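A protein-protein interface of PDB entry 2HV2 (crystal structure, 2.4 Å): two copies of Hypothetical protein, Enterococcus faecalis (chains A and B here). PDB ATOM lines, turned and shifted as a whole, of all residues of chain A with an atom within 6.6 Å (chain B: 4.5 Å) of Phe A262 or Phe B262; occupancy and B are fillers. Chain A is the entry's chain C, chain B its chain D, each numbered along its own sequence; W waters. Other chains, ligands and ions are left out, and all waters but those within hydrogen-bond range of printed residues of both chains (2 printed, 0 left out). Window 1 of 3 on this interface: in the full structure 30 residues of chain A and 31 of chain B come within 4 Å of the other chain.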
ATOM      1  N   PHE A 134      -0.808   7.339  11.918  1.00  0.00           N
ATOM      2  CA  PHE A 134      -0.093   6.320  11.167  1.00  0.00           C
ATOM      3  C   PHE A 134      -0.157   6.574   9.676  1.00  0.00           C
ATOM      4  O   PHE A 134      -1.174   7.078   9.168  1.00  0.00           O
ATOM      5  CB  PHE A 134      -0.712   4.946  11.448  1.00  0.00           C
ATOM      6  CG  PHE A 134      -0.433   4.438  12.812  1.00  0.00           C
ATOM      7  CD1 PHE A 134      -1.432   4.363  13.752  1.00  0.00           C
ATOM      8  CD2 PHE A 134       0.830   4.076  13.159  1.00  0.00           C
ATOM      9  CE1 PHE A 134      -1.170   3.921  15.005  1.00  0.00           C
ATOM     10  CE2 PHE A 134       1.084   3.622  14.427  1.00  0.00           C
ATOM     11  CZ  PHE A 134       0.075   3.541  15.346  1.00  0.00           C
ATOM     12  N   GLU A 135       0.895   6.226   8.921  1.00  0.00           N
ATOM     13  CA  GLU A 135       0.903   6.308   7.461  1.00  0.00           C
ATOM     14  C   GLU A 135       1.401   4.987   6.811  1.00  0.00           C
ATOM     15  O   GLU A 135       2.035   4.162   7.457  1.00  0.00           O
ATOM     16  CB  GLU A 135       1.807   7.450   7.026  1.00  0.00           C
ATOM     17  CG  GLU A 135       1.153   8.819   7.027  1.00  0.00           C
ATOM     18  CD  GLU A 135       2.166   9.956   6.952  1.00  0.00           C
ATOM     19  OE1 GLU A 135       3.350   9.687   6.636  1.00  0.00           O
ATOM     20  OE2 GLU A 135       1.801  11.127   7.245  1.00  0.00           O
ATOM     21  N   GLN A 136       1.137   4.745   5.531  1.00  0.00           N
ATOM     22  CA  GLN A 136       1.697   3.611   4.809  1.00  0.00           C
ATOM     23  C   GLN A 136       2.536   4.032   3.626  1.00  0.00           C
ATOM     24  O   GLN A 136       2.246   5.004   2.972  1.00  0.00           O
ATOM     25  CB  GLN A 136       0.596   2.697   4.305  1.00  0.00           C
ATOM     26  CG  GLN A 136      -0.219   2.085   5.418  1.00  0.00           C
ATOM     27  CD  GLN A 136      -1.169   1.048   4.900  1.00  0.00           C
ATOM     28  OE1 GLN A 136      -1.886   1.328   3.939  1.00  0.00           O
ATOM     29  NE2 GLN A 136      -1.165  -0.167   5.504  1.00  0.00           N
ATOM     30  N   ALA A 137       3.601   3.311   3.314  1.00  0.00           N
ATOM     31  CA  ALA A 137       4.352   3.486   2.085  1.00  0.00           C
ATOM     32  C   ALA A 137       3.918   2.397   1.097  1.00  0.00           C
ATOM     33  O   ALA A 137       3.991   1.199   1.381  1.00  0.00           O
ATOM     34  CB  ALA A 137       5.877   3.444   2.364  1.00  0.00           C
ATOM     35  N   TYR A 139       4.845   0.736  -2.466  1.00  0.00           N
ATOM     36  CA  TYR A 139       5.867   0.595  -3.493  1.00  0.00           C
ATOM     37  C   TYR A 139       5.377  -0.219  -4.675  1.00  0.00           C
ATOM     38  O   TYR A 139       4.744  -1.248  -4.487  1.00  0.00           O
ATOM     39  CB  TYR A 139       7.087  -0.121  -2.952  1.00  0.00           C
ATOM     40  CG  TYR A 139       7.724   0.516  -1.776  1.00  0.00           C
ATOM     41  CD1 TYR A 139       7.209   0.326  -0.504  1.00  0.00           C
ATOM     42  CD2 TYR A 139       8.884   1.255  -1.914  1.00  0.00           C
ATOM     43  CE1 TYR A 139       7.787   0.918   0.595  1.00  0.00           C
ATOM     44  CE2 TYR A 139       9.499   1.826  -0.812  1.00  0.00           C
ATOM     45  CZ  TYR A 139       8.938   1.656   0.435  1.00  0.00           C
ATOM     46  OH  TYR A 139       9.535   2.204   1.532  1.00  0.00           O
ATOM     47  N   ARG A 177      10.784  -2.752  13.725  1.00  0.00           N
ATOM     48  CA  ARG A 177       9.631  -2.049  13.199  1.00  0.00           C
ATOM     49  C   ARG A 177       8.357  -2.474  13.895  1.00  0.00           C
ATOM     50  O   ARG A 177       7.288  -1.903  13.581  1.00  0.00           O
ATOM     51  CB  ARG A 177       9.488  -2.326  11.707  1.00  0.00           C
ATOM     52  CG  ARG A 177      10.783  -2.192  10.922  1.00  0.00           C
ATOM     53  CD  ARG A 177      10.679  -1.291   9.719  1.00  0.00           C
ATOM     54  NE  ARG A 177       9.426  -1.511   9.027  1.00  0.00           N
ATOM     55  CZ  ARG A 177       8.726  -0.565   8.414  1.00  0.00           C
ATOM     56  NH1 ARG A 177       9.154   0.699   8.385  1.00  0.00           N
ATOM     57  NH2 ARG A 177       7.564  -0.893   7.839  1.00  0.00           N
ATOM     58  N   ASN A 260       3.729  -1.203   3.175  1.00  0.00           N
ATOM     59  CA  ASN A 260       4.067  -1.382   4.587  1.00  0.00           C
ATOM     60  C   ASN A 260       3.941  -0.079   5.378  1.00  0.00           C
ATOM     61  O   ASN A 260       3.607   0.948   4.830  1.00  0.00           O
ATOM     62  CB  ASN A 260       5.472  -2.004   4.735  1.00  0.00           C
ATOM     63  CG  ASN A 260       6.593  -1.116   4.203  1.00  0.00           C
ATOM     64  OD1 ASN A 260       6.365  -0.036   3.677  1.00  0.00           O
ATOM     65  ND2 ASN A 260       7.828  -1.571   4.383  1.00  0.00           N
ATOM     66  N   GLY A 261       4.184  -0.075   6.684  1.00  0.00           N
ATOM     67  CA  GLY A 261       4.084   1.103   7.532  1.00  0.00           C
ATOM     68  C   GLY A 261       5.217   2.058   7.227  1.00  0.00           C
ATOM     69  O   GLY A 261       6.368   1.649   6.982  1.00  0.00           O
ATOM     70  N   PHE A 262       4.956   3.352   7.213  1.00  0.00           N
ATOM     71  CA  PHE A 262       5.920   4.332   6.828  1.00  0.00           C
ATOM     72  C   PHE A 262       6.446   5.065   8.052  1.00  0.00           C
ATOM     73  O   PHE A 262       5.678   5.508   8.897  1.00  0.00           O
ATOM     74  CB  PHE A 262       5.251   5.308   5.877  1.00  0.00           C
ATOM     75  CG  PHE A 262       6.164   6.346   5.370  1.00  0.00           C
ATOM     76  CD1 PHE A 262       7.303   5.984   4.694  1.00  0.00           C
ATOM     77  CD2 PHE A 262       5.895   7.665   5.586  1.00  0.00           C
ATOM     78  CE1 PHE A 262       8.158   6.921   4.228  1.00  0.00           C
ATOM     79  CE2 PHE A 262       6.747   8.616   5.120  1.00  0.00           C
ATOM     80  CZ  PHE A 262       7.884   8.244   4.437  1.00  0.00           C
ATOM     81  N   ALA A 263       7.752   5.211   8.209  1.00  0.00           N
ATOM     82  CA  ALA A 263       8.344   5.787   9.404  1.00  0.00           C
ATOM     83  C   ALA A 263       9.208   7.000   9.048  1.00  0.00           C
ATOM     84  O   ALA A 263       9.981   7.475   9.871  1.00  0.00           O
ATOM     85  CB  ALA A 263       9.163   4.726  10.131  1.00  0.00           C
ATOM     86  N   GLY A 264       9.124   7.553   7.850  1.00  0.00           N
ATOM     87  CA  GLY A 264       9.817   8.791   7.518  1.00  0.00           C
ATOM     88  C   GLY A 264      10.827   8.592   6.424  1.00  0.00           C
ATOM     89  O   GLY A 264      11.352   9.563   5.878  1.00  0.00           O
ATOM     90  N   LYS A 265      11.144   7.361   6.037  1.00  0.00           N
ATOM     91  CA  LYS A 265      12.174   7.124   5.064  1.00  0.00           C
ATOM     92  C   LYS A 265      11.837   5.898   4.211  1.00  0.00           C
ATOM     93  O   LYS A 265      11.699   4.786   4.725  1.00  0.00           O
ATOM     94  CB  LYS A 265      13.532   6.947   5.782  1.00  0.00           C
ATOM     95  CG  LYS A 265      14.727   6.875   4.842  1.00  0.00           C
ATOM     96  CD  LYS A 265      15.046   8.226   4.215  1.00  0.00           C
ATOM     97  CE  LYS A 265      15.841   8.115   2.926  1.00  0.00           C
ATOM     98  NZ  LYS A 265      15.240   7.175   1.936  1.00  0.00           N
ATOM     99  N   ASP A 266      11.722   6.037   2.897  1.00  0.00           N
ATOM    100  CA  ASP A 266      11.368   4.914   2.025  1.00  0.00           C
ATOM    101  C   ASP A 266      12.592   4.104   1.646  1.00  0.00           C
ATOM    102  O   ASP A 266      13.729   4.527   1.860  1.00  0.00           O
ATOM    103  CB  ASP A 266      10.623   5.389   0.769  1.00  0.00           C
ATOM    104  CG  ASP A 266      11.498   6.137  -0.207  1.00  0.00           C
ATOM    105  OD1 ASP A 266      10.947   6.991  -0.932  1.00  0.00           O
ATOM    106  OD2 ASP A 266      12.728   5.943  -0.356  1.00  0.00           O
ATOM    107  N   VAL A 278       6.911   5.302  -5.269  1.00  0.00           N
ATOM    108  CA  VAL A 278       6.586   5.331  -3.823  1.00  0.00           C
ATOM    109  C   VAL A 278       5.477   6.345  -3.510  1.00  0.00           C
ATOM    110  O   VAL A 278       5.636   7.529  -3.725  1.00  0.00           O
ATOM    111  CB  VAL A 278       7.811   5.691  -2.950  1.00  0.00           C
ATOM    112  CG1 VAL A 278       7.445   5.681  -1.470  1.00  0.00           C
ATOM    113  CG2 VAL A 278       8.970   4.748  -3.217  1.00  0.00           C
ATOM    114  N   ILE A 280       2.758   7.804  -0.430  1.00  0.00           N
ATOM    115  CA  ILE A 280       2.494   7.788   1.008  1.00  0.00           C
ATOM    116  C   ILE A 280       1.004   7.822   1.277  1.00  0.00           C
ATOM    117  O   ILE A 280       0.307   8.731   0.856  1.00  0.00           O
ATOM    118  CB  ILE A 280       3.191   8.946   1.738  1.00  0.00           C
ATOM    119  CG1 ILE A 280       4.697   8.955   1.440  1.00  0.00           C
ATOM    120  CG2 ILE A 280       2.972   8.801   3.226  1.00  0.00           C
ATOM    121  CD1 ILE A 280       5.319   7.559   1.302  1.00  0.00           C
ATOM    122  N   LEU A 281       0.452   6.839   1.967  1.00  0.00           N
ATOM    123  CA  LEU A 281      -0.972   6.732   2.172  1.00  0.00           C
ATOM    124  C   LEU A 281      -1.360   7.072   3.614  1.00  0.00           C
ATOM    125  O   LEU A 281      -0.735   6.609   4.558  1.00  0.00           O
ATOM    126  CB  LEU A 281      -1.448   5.307   1.860  1.00  0.00           C
ATOM    127  CG  LEU A 281      -1.120   4.709   0.491  1.00  0.00           C
ATOM    128  CD1 LEU A 281      -1.637   3.258   0.419  1.00  0.00           C
ATOM    129  CD2 LEU A 281      -1.714   5.533  -0.595  1.00  0.00           C
ATOM    130  N   MET A 393       8.578   8.055  14.171  1.00  0.00           N
ATOM    131  CA  MET A 393       7.159   7.889  14.011  1.00  0.00           C
ATOM    132  C   MET A 393       6.717   6.491  14.403  1.00  0.00           C
ATOM    133  O   MET A 393       7.469   5.527  14.270  1.00  0.00           O
ATOM    134  CB  MET A 393       6.775   8.135  12.558  1.00  0.00           C
ATOM    135  CG  MET A 393       7.097   9.522  12.101  1.00  0.00           C
ATOM    136  SD  MET A 393       6.739   9.753  10.198  1.00  0.00           S
ATOM    137  CE  MET A 393       4.810   9.332  10.128  1.00  0.00           C
ATOM    138  N   PRO A 394       5.478   6.379  14.859  1.00  0.00           N
ATOM    139  CA  PRO A 394       4.916   5.087  15.185  1.00  0.00           C
ATOM    140  C   PRO A 394       4.631   4.242  13.939  1.00  0.00           C
ATOM    141  O   PRO A 394       4.301   4.788  12.877  1.00  0.00           O
ATOM    142  CB  PRO A 394       3.618   5.453  15.932  1.00  0.00           C
ATOM    143  CG  PRO A 394       3.219   6.772  15.383  1.00  0.00           C
ATOM    144  CD  PRO A 394       4.517   7.477  15.085  1.00  0.00           C
ATOM    145  N   ILE A 395       4.735   2.915  14.013  1.00  0.00           N
ATOM    146  CA  ILE A 395       4.524   2.017  12.889  1.00  0.00           C
ATOM    147  C   ILE A 395       3.459   0.969  13.258  1.00  0.00           C
ATOM    148  O   ILE A 395       3.592   0.265  14.261  1.00  0.00           O
ATOM    149  CB  ILE A 395       5.840   1.321  12.505  1.00  0.00           C
ATOM    150  CG1 ILE A 395       6.945   2.351  12.189  1.00  0.00           C
ATOM    151  CG2 ILE A 395       5.604   0.372  11.323  1.00  0.00           C
ATOM    152  CD1 ILE A 395       8.368   1.808  12.332  1.00  0.00           C
ATOM    153  N   LEU A 396       2.385   0.837  12.480  1.00  0.00           N
ATOM    154  CA  LEU A 396       1.372  -0.201  12.629  1.00  0.00           C
ATOM    155  C   LEU A 396       1.351  -1.047  11.369  1.00  0.00           C
ATOM    156  O   LEU A 396       1.165  -0.523  10.289  1.00  0.00           O
ATOM    157  CB  LEU A 396       0.014   0.448  12.828  1.00  0.00           C
ATOM    158  CG  LEU A 396      -1.189  -0.440  13.023  1.00  0.00           C
ATOM    159  CD1 LEU A 396      -0.985  -1.408  14.217  1.00  0.00           C
ATOM    160  CD2 LEU A 396      -2.422   0.445  13.206  1.00  0.00           C
ATOM    161  N   GLU A 397       1.559  -2.357  11.440  1.00  0.00           N
ATOM    162  CA  GLU A 397       1.485  -3.251  10.293  1.00  0.00           C
ATOM    163  C   GLU A 397       0.402  -4.296  10.539  1.00  0.00           C
ATOM    164  O   GLU A 397       0.560  -5.466  10.220  1.00  0.00           O
ATOM    165  CB  GLU A 397       2.848  -3.877  10.031  1.00  0.00           C
ATOM    166  CG  GLU A 397       3.945  -2.820  10.038  1.00  0.00           C
ATOM    167  CD  GLU A 397       5.055  -3.062   9.039  1.00  0.00           C
ATOM    168  OE1 GLU A 397       5.950  -3.902   9.331  1.00  0.00           O
ATOM    169  OE2 GLU A 397       5.053  -2.372   7.994  1.00  0.00           O
ATOM    170  N   GLU B 135      15.369  14.087  -1.501  1.00  0.00           N
ATOM    171  CA  GLU B 135      14.105  13.514  -1.989  1.00  0.00           C
ATOM    172  C   GLU B 135      13.095  14.644  -2.205  1.00  0.00           C
ATOM    173  O   GLU B 135      13.259  15.711  -1.665  1.00  0.00           O
ATOM    174  CB  GLU B 135      13.581  12.450  -1.007  1.00  0.00           C
ATOM    175  CG  GLU B 135      14.005  11.018  -1.352  1.00  0.00           C
ATOM    176  CD  GLU B 135      13.917  10.022  -0.164  1.00  0.00           C
ATOM    177  OE1 GLU B 135      13.182  10.270   0.840  1.00  0.00           O
ATOM    178  OE2 GLU B 135      14.594   8.955  -0.223  1.00  0.00           O
ATOM    179  N   GLN B 136      12.080  14.502  -3.043  1.00  0.00           N
ATOM    180  CA  GLN B 136      11.051  15.510  -3.221  1.00  0.00           C
ATOM    181  C   GLN B 136       9.662  14.935  -2.912  1.00  0.00           C
ATOM    182  O   GLN B 136       9.441  13.759  -3.125  1.00  0.00           O
ATOM    183  CB  GLN B 136      11.062  16.007  -4.653  1.00  0.00           C
ATOM    184  CG  GLN B 136      12.194  16.975  -4.977  1.00  0.00           C
ATOM    185  CD  GLN B 136      12.064  17.517  -6.391  1.00  0.00           C
ATOM    186  OE1 GLN B 136      11.777  16.748  -7.334  1.00  0.00           O
ATOM    187  NE2 GLN B 136      12.242  18.829  -6.549  1.00  0.00           N
ATOM    188  N   ALA B 137       8.697  15.708  -2.406  1.00  0.00           N
ATOM    189  CA  ALA B 137       7.304  15.254  -2.227  1.00  0.00           C
ATOM    190  C   ALA B 137       6.435  15.833  -3.354  1.00  0.00           C
ATOM    191  O   ALA B 137       6.457  17.047  -3.604  1.00  0.00           O
ATOM    192  CB  ALA B 137       6.766  15.683  -0.853  1.00  0.00           C
ATOM    193  N   ASN B 260       7.920  19.865  -3.668  1.00  0.00           N
ATOM    194  CA  ASN B 260       8.868  20.559  -2.819  1.00  0.00           C
ATOM    195  C   ASN B 260       9.827  19.591  -2.118  1.00  0.00           C
ATOM    196  O   ASN B 260       9.735  18.392  -2.296  1.00  0.00           O
ATOM    197  CB  ASN B 260       8.105  21.455  -1.833  1.00  0.00           C
ATOM    198  CG  ASN B 260       7.432  20.694  -0.708  1.00  0.00           C
ATOM    199  OD1 ASN B 260       7.251  19.473  -0.739  1.00  0.00           O
ATOM    200  ND2 ASN B 260       7.075  21.426   0.314  1.00  0.00           N
ATOM    201  N   GLY B 261      10.779  20.055  -1.324  1.00  0.00           N
ATOM    202  CA  GLY B 261      11.736  19.195  -0.653  1.00  0.00           C
ATOM    203  C   GLY B 261      11.104  18.317   0.407  1.00  0.00           C
ATOM    204  O   GLY B 261      10.388  18.815   1.269  1.00  0.00           O
ATOM    205  N   PHE B 262      11.332  17.008   0.412  1.00  0.00           N
ATOM    206  CA  PHE B 262      10.767  16.090   1.401  1.00  0.00           C
ATOM    207  C   PHE B 262      11.764  15.837   2.497  1.00  0.00           C
ATOM    208  O   PHE B 262      12.879  15.388   2.208  1.00  0.00           O
ATOM    209  CB  PHE B 262      10.426  14.760   0.744  1.00  0.00           C
ATOM    210  CG  PHE B 262       9.794  13.745   1.682  1.00  0.00           C
ATOM    211  CD1 PHE B 262       8.557  13.984   2.251  1.00  0.00           C
ATOM    212  CD2 PHE B 262      10.423  12.541   1.952  1.00  0.00           C
ATOM    213  CE1 PHE B 262       7.977  13.054   3.074  1.00  0.00           C
ATOM    214  CE2 PHE B 262       9.830  11.608   2.776  1.00  0.00           C
ATOM    215  CZ  PHE B 262       8.609  11.866   3.339  1.00  0.00           C
ATOM    216  N   ALA B 263      11.428  16.098   3.767  1.00  0.00           N
ATOM    217  CA  ALA B 263      12.294  15.810   4.919  1.00  0.00           C
ATOM    218  C   ALA B 263      11.629  14.812   5.896  1.00  0.00           C
ATOM    219  O   ALA B 263      11.883  14.847   7.110  1.00  0.00           O
ATOM    220  CB  ALA B 263      12.696  17.103   5.643  1.00  0.00           C
ATOM    221  N   GLY B 264      10.800  13.882   5.427  1.00  0.00           N
ATOM    222  CA  GLY B 264      10.376  12.734   6.223  1.00  0.00           C
ATOM    223  C   GLY B 264       8.954  12.846   6.725  1.00  0.00           C
ATOM    224  O   GLY B 264       8.406  11.883   7.247  1.00  0.00           O
ATOM    225  N   LYS B 265       8.299  13.990   6.611  1.00  0.00           N
ATOM    226  CA  LYS B 265       6.936  14.148   7.055  1.00  0.00           C
ATOM    227  C   LYS B 265       6.203  14.974   6.025  1.00  0.00           C
ATOM    228  O   LYS B 265       6.578  16.094   5.771  1.00  0.00           O
ATOM    229  CB  LYS B 265       6.903  14.832   8.429  1.00  0.00           C
ATOM    230  CG  LYS B 265       5.535  14.860   9.095  1.00  0.00           C
ATOM    231  CD  LYS B 265       5.138  13.507   9.668  1.00  0.00           C
ATOM    232  CE  LYS B 265       3.647  13.234   9.539  1.00  0.00           C
ATOM    233  NZ  LYS B 265       3.123  13.427   8.156  1.00  0.00           N
ATOM    234  N   ASP B 266       5.152  14.469   5.397  1.00  0.00           N
ATOM    235  CA  ASP B 266       4.387  15.218   4.415  1.00  0.00           C
ATOM    236  C   ASP B 266       3.247  16.006   5.077  1.00  0.00           C
ATOM    237  O   ASP B 266       2.881  15.732   6.219  1.00  0.00           O
ATOM    238  CB  ASP B 266       3.850  14.267   3.322  1.00  0.00           C
ATOM    239  CG  ASP B 266       2.856  13.217   3.856  1.00  0.00           C
ATOM    240  OD1 ASP B 266       3.242  12.316   4.648  1.00  0.00           O
ATOM    241  OD2 ASP B 266       1.668  13.211   3.507  1.00  0.00           O
ATOM    242  N   ILE B 280       6.874  10.260  -3.365  1.00  0.00           N
ATOM    243  CA  ILE B 280       8.214  10.673  -3.016  1.00  0.00           C
ATOM    244  C   ILE B 280       9.131  10.363  -4.175  1.00  0.00           C
ATOM    245  O   ILE B 280       9.236   9.206  -4.634  1.00  0.00           O
ATOM    246  CB  ILE B 280       8.673  10.020  -1.717  1.00  0.00           C
ATOM    247  CG1 ILE B 280       7.668  10.338  -0.625  1.00  0.00           C
ATOM    248  CG2 ILE B 280      10.064  10.507  -1.289  1.00  0.00           C
ATOM    249  CD1 ILE B 280       7.903   9.445   0.567  1.00  0.00           C
ATOM    250  N   MET B 393      16.768  15.288   7.885  1.00  0.00           N
ATOM    251  CA  MET B 393      17.224  15.167   6.513  1.00  0.00           C
ATOM    252  C   MET B 393      17.505  16.507   5.865  1.00  0.00           C
ATOM    253  O   MET B 393      16.887  17.522   6.194  1.00  0.00           O
ATOM    254  CB  MET B 393      16.185  14.444   5.662  1.00  0.00           C
ATOM    255  CG  MET B 393      16.060  12.977   5.951  1.00  0.00           C
ATOM    256  SD  MET B 393      14.406  12.257   5.189  1.00  0.00           S
ATOM    257  CE  MET B 393      14.677  12.550   3.259  1.00  0.00           C
HETATM  258  O   HOH W   1      11.285   7.420  -3.424  1.00  0.00           O
HETATM  259  O   HOH W   2       7.933   7.741  -6.697  1.00  0.00           O
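Of the 21 printed residues of chain A, 7 touch a printed residue of chain B. Printed residues of chain A that touch a printed residue of chain B: Glu A135, Phe A262, Gly A264, Lys A265, Asp A266, Val A278 and Ile A280. Hydrophobic or aromatic side chains of chain A within 4 Å of the printed part of chain B: Phe A262 and Ile A280. Among the printed residues, Asp or Glu carboxylates within 4 Å of a Lys or Arg side-chain nitrogen of the other chain: Glu A135 with Lys B265 and Lys A265 with Glu B135.
The backbone carbonyl oxygen (O) of Glu A135 is in hydrogen-bond range of the backbone NH (N) of Phe A262 (3.0 Å). The side-chain amino group (NZ) of Lys A265 lies within salt-bridge range of the side-chain carboxylate (OD2) of Asp A266. O of Glu B135 is in hydrogen-bond range of N of Phe B262 (3.1 Å). The side-chain carboxylate (OD1) of Asp B266 lies within salt-bridge range of the side-chain amino group (NZ) of Lys B265 (3.7 Å).
OE2 of Glu A135 lies within salt-bridge range of NZ of Lys B265 (2.8 Å). The side-chain carboxylate (OE2) of Glu B135 is in salt-bridge range of the side-chain amino group (NZ) of Lys A265 (2.9 Å). O of Val A278 lies within hydrogen-bond range of N of Ile B280. OE2 of Glu A135 sits close to OD1 of Asp B266 (3.2 Å).
Gln A136 touches none of the printed residues of chain B. Phe A262 touches just one residue of chain B: Phe B262. Printed residues of chain B within 4 Å of Val A278: Ile B280. Printed residues of chain B within 4 Å of Ile A280: Asp B266 (3.8 Å) and Ile B280 (3.3 Å). Of the printed residues of chain A, Phe B262 touches Phe A262 (3.9 Å). The nearest residue of chain B that does not touch Phe A262 is Ile B280 (4.1 Å).
CZ of Phe A262 touches CZ of Phe B262 (3.9 Å). Gly B264 touches Gly A264. OD2 of Asp A266 touches OE2 of Glu B135, 3.5 Å away. Asp A266 touches Ile B280. Ile A280 touches Asp B266 (CG2 to OD1, 3.8 Å). CD1 of Ile A280 touches CD1 of Ile B280, 3.3 Å away.
Water W1 bridges OD1 of Asp A266 (2.6 Å) and O of Ile B280 (3.0 Å). Water W2 bridges O of Ile B280 (2.8 Å) and N of Val A278 (3.0 Å).
Glu A135 touches Lys B265, and with the chains exchanged Lys A265 touches Glu B135. Glu A135 touches Asp B266, and with the chains exchanged Asp A266 touches Glu B135. Gly A264 touches its own counterpart, Gly B264. Asp A266 touches Ile B280, and with the chains exchanged Ile A280 touches Asp B266.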
